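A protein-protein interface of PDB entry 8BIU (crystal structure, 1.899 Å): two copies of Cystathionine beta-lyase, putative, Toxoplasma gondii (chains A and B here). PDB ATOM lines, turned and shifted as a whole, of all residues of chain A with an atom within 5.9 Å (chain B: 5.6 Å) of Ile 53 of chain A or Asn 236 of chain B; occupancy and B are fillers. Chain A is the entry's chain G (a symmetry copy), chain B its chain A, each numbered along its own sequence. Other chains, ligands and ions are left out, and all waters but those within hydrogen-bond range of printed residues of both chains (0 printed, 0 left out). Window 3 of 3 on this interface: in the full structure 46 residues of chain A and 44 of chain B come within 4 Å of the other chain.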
ATOM      1  N   VAL A  44      -6.633  -5.027 -29.538  1.00  0.00           N
ATOM      2  CA  VAL A  44      -5.803  -5.467 -28.428  1.00  0.00           C
ATOM      3  C   VAL A  44      -4.585  -4.563 -28.325  1.00  0.00           C
ATOM      4  O   VAL A  44      -4.047  -4.098 -29.335  1.00  0.00           O
ATOM      5  CB  VAL A  44      -5.387  -6.946 -28.579  1.00  0.00           C
ATOM      6  CG1 VAL A  44      -4.449  -7.353 -27.458  1.00  0.00           C
ATOM      7  CG2 VAL A  44      -6.623  -7.828 -28.610  1.00  0.00           C
ATOM      8  N   GLU A  45      -4.178  -4.291 -27.098  1.00  0.00           N
ATOM      9  CA  GLU A  45      -2.959  -3.578 -26.790  1.00  0.00           C
ATOM     10  C   GLU A  45      -2.245  -4.350 -25.690  1.00  0.00           C
ATOM     11  O   GLU A  45      -2.867  -5.161 -25.006  1.00  0.00           O
ATOM     12  CB  GLU A  45      -3.254  -2.143 -26.329  1.00  0.00           C
ATOM     13  CG  GLU A  45      -4.044  -2.062 -25.027  1.00  0.00           C
ATOM     14  CD  GLU A  45      -3.979  -0.678 -24.385  1.00  0.00           C
ATOM     15  OE1 GLU A  45      -2.976  -0.377 -23.699  1.00  0.00           O
ATOM     16  OE2 GLU A  45      -4.929   0.116 -24.581  1.00  0.00           O
ATOM     17  N   PRO A  46      -0.947  -4.132 -25.516  1.00  0.00           N
ATOM     18  CA  PRO A  46      -0.271  -4.743 -24.368  1.00  0.00           C
ATOM     19  C   PRO A  46      -0.989  -4.391 -23.076  1.00  0.00           C
ATOM     20  O   PRO A  46      -1.526  -3.291 -22.913  1.00  0.00           O
ATOM     21  CB  PRO A  46       1.136  -4.144 -24.423  1.00  0.00           C
ATOM     22  CG  PRO A  46       1.321  -3.778 -25.851  1.00  0.00           C
ATOM     23  CD  PRO A  46      -0.022  -3.364 -26.363  1.00  0.00           C
ATOM     24  N   ASP A  47      -1.011  -5.348 -22.164  1.00  0.00           N
ATOM     25  CA  ASP A  47      -1.662  -5.170 -20.882  1.00  0.00           C
ATOM     26  C   ASP A  47      -1.090  -3.947 -20.161  1.00  0.00           C
ATOM     27  O   ASP A  47       0.117  -3.911 -19.878  1.00  0.00           O
ATOM     28  CB  ASP A  47      -1.477  -6.429 -20.040  1.00  0.00           C
ATOM     29  CG  ASP A  47      -1.928  -6.243 -18.611  1.00  0.00           C
ATOM     30  OD1 ASP A  47      -3.062  -5.749 -18.402  1.00  0.00           O
ATOM     31  OD2 ASP A  47      -1.152  -6.583 -17.695  1.00  0.00           O
ATOM     32  N   GLY A  51       2.349  -4.958 -19.325  1.00  0.00           N
ATOM     33  CA  GLY A  51       2.920  -4.970 -20.654  1.00  0.00           C
ATOM     34  C   GLY A  51       2.775  -6.284 -21.388  1.00  0.00           C
ATOM     35  O   GLY A  51       3.309  -6.418 -22.492  1.00  0.00           O
ATOM     36  N   ALA A  52       2.077  -7.258 -20.809  1.00  0.00           N
ATOM     37  CA  ALA A  52       1.859  -8.548 -21.452  1.00  0.00           C
ATOM     38  C   ALA A  52       1.401  -8.356 -22.889  1.00  0.00           C
ATOM     39  O   ALA A  52       0.398  -7.682 -23.149  1.00  0.00           O
ATOM     40  CB  ALA A  52       0.817  -9.355 -20.671  1.00  0.00           C
ATOM     41  N   ILE A  53       2.136  -8.961 -23.825  1.00  0.00           N
ATOM     42  CA  ILE A  53       1.850  -8.695 -25.229  1.00  0.00           C
ATOM     43  C   ILE A  53       0.504  -9.295 -25.631  1.00  0.00           C
ATOM     44  O   ILE A  53      -0.174  -8.773 -26.529  1.00  0.00           O
ATOM     45  CB  ILE A  53       3.015  -9.179 -26.119  1.00  0.00           C
ATOM     46  CG1 ILE A  53       2.956  -8.498 -27.485  1.00  0.00           C
ATOM     47  CG2 ILE A  53       3.031 -10.682 -26.265  1.00  0.00           C
ATOM     48  CD1 ILE A  53       4.083  -8.893 -28.410  1.00  0.00           C
ATOM     49  N   LEU A  54       0.066 -10.375 -24.956  1.00  0.00           N
ATOM     50  CA  LEU A  54      -1.287 -10.886 -25.136  1.00  0.00           C
ATOM     51  C   LEU A  54      -2.174 -10.487 -23.954  1.00  0.00           C
ATOM     52  O   LEU A  54      -1.695 -10.422 -22.818  1.00  0.00           O
ATOM     53  CB  LEU A  54      -1.276 -12.412 -25.260  1.00  0.00           C
ATOM     54  CG  LEU A  54      -0.280 -13.035 -26.238  1.00  0.00           C
ATOM     55  CD1 LEU A  54      -0.479 -14.527 -26.309  1.00  0.00           C
ATOM     56  CD2 LEU A  54      -0.438 -12.433 -27.617  1.00  0.00           C
ATOM     57  N   PRO A  55      -3.463 -10.256 -24.163  1.00  0.00           N
ATOM     58  CA  PRO A  55      -4.339  -9.970 -23.029  1.00  0.00           C
ATOM     59  C   PRO A  55      -4.482 -11.195 -22.144  1.00  0.00           C
ATOM     60  O   PRO A  55      -4.713 -12.304 -22.645  1.00  0.00           O
ATOM     61  CB  PRO A  55      -5.673  -9.598 -23.693  1.00  0.00           C
ATOM     62  CG  PRO A  55      -5.616 -10.157 -25.093  1.00  0.00           C
ATOM     63  CD  PRO A  55      -4.221 -10.668 -25.357  1.00  0.00           C
ATOM     64  N   THR B 229       9.111 -22.169 -27.618  1.00  0.00           N
ATOM     65  CA  THR B 229       8.575 -20.842 -27.326  1.00  0.00           C
ATOM     66  C   THR B 229       8.488 -19.975 -28.578  1.00  0.00           C
ATOM     67  O   THR B 229       7.517 -19.238 -28.772  1.00  0.00           O
ATOM     68  CB  THR B 229       9.456 -20.144 -26.286  1.00  0.00           C
ATOM     69  OG1 THR B 229       9.717 -21.030 -25.186  1.00  0.00           O
ATOM     70  CG2 THR B 229       8.804 -18.859 -25.793  1.00  0.00           C
ATOM     71  N   ASP B 233       5.598 -22.432 -31.251  1.00  0.00           N
ATOM     72  CA  ASP B 233       4.510 -21.598 -30.752  1.00  0.00           C
ATOM     73  C   ASP B 233       4.220 -20.479 -31.741  1.00  0.00           C
ATOM     74  O   ASP B 233       3.147 -20.435 -32.354  1.00  0.00           O
ATOM     75  CB  ASP B 233       4.885 -21.027 -29.377  1.00  0.00           C
ATOM     76  CG  ASP B 233       3.748 -20.258 -28.698  1.00  0.00           C
ATOM     77  OD1 ASP B 233       2.995 -19.526 -29.357  1.00  0.00           O
ATOM     78  OD2 ASP B 233       3.616 -20.372 -27.469  1.00  0.00           O
ATOM     79  N   GLY B 234       5.185 -19.578 -31.906  1.00  0.00           N
ATOM     80  CA  GLY B 234       5.028 -18.457 -32.806  1.00  0.00           C
ATOM     81  C   GLY B 234       3.881 -17.536 -32.481  1.00  0.00           C
ATOM     82  O   GLY B 234       3.515 -16.701 -33.312  1.00  0.00           O
ATOM     83  N   HIS B 235       3.300 -17.654 -31.295  1.00  0.00           N
ATOM     84  CA  HIS B 235       2.157 -16.837 -30.928  1.00  0.00           C
ATOM     85  C   HIS B 235       2.348 -16.113 -29.600  1.00  0.00           C
ATOM     86  O   HIS B 235       1.403 -15.493 -29.111  1.00  0.00           O
ATOM     87  CB  HIS B 235       0.892 -17.696 -30.867  1.00  0.00           C
ATOM     88  CG  HIS B 235       0.445 -18.226 -32.194  1.00  0.00           C
ATOM     89  ND1 HIS B 235       1.092 -19.256 -32.844  1.00  0.00           N
ATOM     90  CD2 HIS B 235      -0.593 -17.879 -32.988  1.00  0.00           C
ATOM     91  CE1 HIS B 235       0.469 -19.525 -33.977  1.00  0.00           C
ATOM     92  NE2 HIS B 235      -0.560 -18.704 -34.085  1.00  0.00           N
ATOM     93  N   ASN B 236       3.538 -16.168 -29.006  1.00  0.00           N
ATOM     94  CA  ASN B 236       3.811 -15.495 -27.742  1.00  0.00           C
ATOM     95  C   ASN B 236       2.956 -16.059 -26.624  1.00  0.00           C
ATOM     96  O   ASN B 236       2.642 -15.373 -25.647  1.00  0.00           O
ATOM     97  CB  ASN B 236       3.587 -13.989 -27.850  1.00  0.00           C
ATOM     98  CG  ASN B 236       4.723 -13.297 -28.530  1.00  0.00           C
ATOM     99  OD1 ASN B 236       5.882 -13.478 -28.149  1.00  0.00           O
ATOM    100  ND2 ASN B 236       4.415 -12.493 -29.540  1.00  0.00           N
ATOM    101  N   CYS B 237       2.570 -17.312 -26.790  1.00  0.00           N
ATOM    102  CA  CYS B 237       1.596 -17.960 -25.936  1.00  0.00           C
ATOM    103  C   CYS B 237       2.249 -18.815 -24.860  1.00  0.00           C
ATOM    104  O   CYS B 237       2.026 -18.587 -23.670  1.00  0.00           O
ATOM    105  CB  CYS B 237       0.667 -18.813 -26.802  1.00  0.00           C
ATOM    106  SG  CYS B 237      -0.553 -19.706 -25.890  1.00  0.00           S
ATOM    107  N   THR B 238       3.059 -19.792 -25.247  1.00  0.00           N
ATOM    108  CA  THR B 238       3.624 -20.725 -24.291  1.00  0.00           C
ATOM    109  C   THR B 238       5.140 -20.622 -24.277  1.00  0.00           C
ATOM    110  O   THR B 238       5.773 -20.136 -25.219  1.00  0.00           O
ATOM    111  CB  THR B 238       3.247 -22.192 -24.594  1.00  0.00           C
ATOM    112  OG1 THR B 238       3.935 -22.646 -25.766  1.00  0.00           O
ATOM    113  CG2 THR B 238       1.749 -22.368 -24.812  1.00  0.00           C
ATOM    114  N   SER B 356       6.440  -4.111 -31.412  1.00  0.00           N
ATOM    115  CA  SER B 356       6.472  -4.248 -29.962  1.00  0.00           C
ATOM    116  C   SER B 356       7.913  -4.242 -29.481  1.00  0.00           C
ATOM    117  O   SER B 356       8.757  -4.958 -30.021  1.00  0.00           O
ATOM    118  CB  SER B 356       5.796  -5.541 -29.497  1.00  0.00           C
ATOM    119  OG  SER B 356       4.428  -5.568 -29.861  1.00  0.00           O
ATOM    120  N   CYS B 358      10.138  -5.507 -26.934  1.00  0.00           N
ATOM    121  CA  CYS B 358      10.101  -6.548 -25.920  1.00  0.00           C
ATOM    122  C   CYS B 358      11.120  -7.609 -26.292  1.00  0.00           C
ATOM    123  O   CYS B 358      11.851  -7.474 -27.276  1.00  0.00           O
ATOM    124  CB  CYS B 358       8.686  -7.099 -25.779  1.00  0.00           C
ATOM    125  SG  CYS B 358       8.095  -7.915 -27.204  1.00  0.00           S
ATOM    126  N   GLU B 359      11.185  -8.655 -25.472  1.00  0.00           N
ATOM    127  CA  GLU B 359      12.023  -9.812 -25.741  1.00  0.00           C
ATOM    128  C   GLU B 359      11.203 -10.840 -26.512  1.00  0.00           C
ATOM    129  O   GLU B 359      10.042 -10.610 -26.853  1.00  0.00           O
ATOM    130  CB  GLU B 359      12.587 -10.366 -24.434  1.00  0.00           C
ATOM    131  CG  GLU B 359      13.499  -9.396 -23.697  1.00  0.00           C
ATOM    132  CD  GLU B 359      14.403 -10.085 -22.683  1.00  0.00           C
ATOM    133  OE1 GLU B 359      15.617  -9.777 -22.653  1.00  0.00           O
ATOM    134  OE2 GLU B 359      13.895 -10.925 -21.905  1.00  0.00           O
ATOM    135  N   ASN B 360      11.806 -11.989 -26.790  1.00  0.00           N
ATOM    136  CA  ASN B 360      11.186 -13.046 -27.581  1.00  0.00           C
ATOM    137  C   ASN B 360      11.239 -12.740 -29.073  1.00  0.00           C
ATOM    138  O   ASN B 360      11.691 -11.661 -29.483  1.00  0.00           O
ATOM    139  CB  ASN B 360       9.738 -13.305 -27.158  1.00  0.00           C
ATOM    140  CG  ASN B 360       9.297 -14.719 -27.479  1.00  0.00           C
ATOM    141  OD1 ASN B 360      10.125 -15.637 -27.518  1.00  0.00           O
ATOM    142  ND2 ASN B 360       7.999 -14.910 -27.704  1.00  0.00           N
ATOM    143  N   LEU B 361      10.787 -13.698 -29.882  1.00  0.00           N
ATOM    144  CA  LEU B 361      10.959 -13.655 -31.324  1.00  0.00           C
ATOM    145  C   LEU B 361      10.247 -14.857 -31.921  1.00  0.00           C
ATOM    146  O   LEU B 361       9.877 -15.791 -31.213  1.00  0.00           O
ATOM    147  CB  LEU B 361      12.440 -13.669 -31.693  1.00  0.00           C
ATOM    148  CG  LEU B 361      13.190 -14.889 -31.150  1.00  0.00           C
ATOM    149  CD1 LEU B 361      13.328 -16.007 -32.189  1.00  0.00           C
ATOM    150  CD2 LEU B 361      14.528 -14.468 -30.596  1.00  0.00           C
ATOM    151  N   ALA B 363       7.311 -14.764 -33.270  1.00  0.00           N
ATOM    152  CA  ALA B 363       5.872 -14.653 -33.114  1.00  0.00           C
ATOM    153  C   ALA B 363       5.226 -13.929 -34.293  1.00  0.00           C
ATOM    154  O   ALA B 363       5.865 -13.177 -35.028  1.00  0.00           O
ATOM    155  CB  ALA B 363       5.546 -13.924 -31.813  1.00  0.00           C
ATOM    156  N   CYS B 364       3.930 -14.187 -34.474  1.00  0.00           N
ATOM    157  CA  CYS B 364       3.133 -13.386 -35.395  1.00  0.00           C
ATOM    158  C   CYS B 364       3.337 -11.896 -35.178  1.00  0.00           C
ATOM    159  O   CYS B 364       3.254 -11.120 -36.131  1.00  0.00           O
ATOM    160  CB  CYS B 364       1.634 -13.695 -35.254  1.00  0.00           C
ATOM    161  SG  CYS B 364       1.087 -15.404 -35.489  1.00  0.00           S
ATOM    162  N   GLU B 365       3.568 -11.472 -33.938  1.00  0.00           N
ATOM    163  CA  GLU B 365       3.745 -10.058 -33.651  1.00  0.00           C
ATOM    164  C   GLU B 365       5.195  -9.692 -33.913  1.00  0.00           C
ATOM    165  O   GLU B 365       6.109 -10.336 -33.388  1.00  0.00           O
ATOM    166  CB  GLU B 365       3.360  -9.754 -32.213  1.00  0.00           C
ATOM    167  CG  GLU B 365       1.907 -10.040 -31.960  1.00  0.00           C
ATOM    168  CD  GLU B 365       1.677 -11.491 -31.584  1.00  0.00           C
ATOM    169  OE1 GLU B 365       2.646 -12.280 -31.610  1.00  0.00           O
ATOM    170  OE2 GLU B 365       0.528 -11.853 -31.278  1.00  0.00           O
ATOM    171  N   ILE B 367       8.565  -7.887 -33.421  1.00  0.00           N
ATOM    172  CA  ILE B 367       9.234  -7.511 -32.189  1.00  0.00           C
ATOM    173  C   ILE B 367      10.564  -6.881 -32.541  1.00  0.00           C
ATOM    174  O   ILE B 367      11.242  -7.308 -33.480  1.00  0.00           O
ATOM    175  CB  ILE B 367       9.449  -8.725 -31.265  1.00  0.00           C
ATOM    176  CG1 ILE B 367       8.128  -9.165 -30.640  1.00  0.00           C
ATOM    177  CG2 ILE B 367      10.501  -8.417 -30.201  1.00  0.00           C
ATOM    178  CD1 ILE B 367       8.141 -10.604 -30.156  1.00  0.00           C
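Among the printed residues, pairs that only touch across the chains: Leu 54 of chain A with Asn 236 of chain B, Leu 54 of chain A with His 235 of chain B, Ile 53 of chain A with Ser 356 of chain B, Ile 53 of chain A with Asn 236 of chain B, Leu 54 of chain A with Glu 365 of chain B and Ile 53 of chain A with Glu 365 of chain B.
Of the printed residues of chain B, Ile 53 of chain A touches Asn 236, Ser 356 and Glu 365.
Printed residues of chain B within 4 Å of Leu 54 of chain A: His 235 (3.5 Å), Asn 236 (3.3 Å) and Glu 365 (3.8 Å).
Of the printed residues of chain A, His 235 of chain B touches Leu 54.
Asn 236 of chain B touches just these residues of chain A: Ile 53 (3.7 Å) and Leu 54 (3.3 Å).
Of the printed residues of chain A, Ser 356 of chain B touches Ile 53.
Of the printed residues of chain A, Glu 365 of chain B touches Ile 53 and Leu 54.
The nearest residue of chain B that does not touch Ile 53 of chain A is Cys 358 of chain B (4.3 Å).
The nearest printed residue of chain A that does not touch Asn 236 of chain B is Ala 52 of chain A (7.6 Å).
Of the 9 printed residues of chain A, 2 touch a printed residue of chain B.
Printed residues of chain A that touch a printed residue of chain B: Ile 53 and Leu 54.
Of the 16 printed residues of chain B, 4 touch a printed residue of chain A.
Printed residues of chain B that touch a printed residue of chain A: His 235, Asn 236, Ser 356 and Glu 365.
Among the printed residues, no Asp or Glu carboxylate lies within 4 Å of a Lys or Arg side-chain nitrogen of the other chain.
N of Asn 236 of chain B lies within hydrogen-bond range of OD1 of Asp 233 of chain B (3.4 Å).
ND2 of Asn 236 of chain B lies within hydrogen-bond range of OE1 of Glu 365 of chain B.
O of Asp 233 of chain B is in hydrogen-bond range of ND1 of His 235 of chain B (2.4 Å).
ND2 of Asn 360 of chain B sits at hydrogen-bond distance from OD1 of Asn 236 of chain B, at 2.6 Å.
No position is printed for both chains.
Of the 6 pairs that touch across the chains among the printed residues, none has its exchanged pair printed and touching as well.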
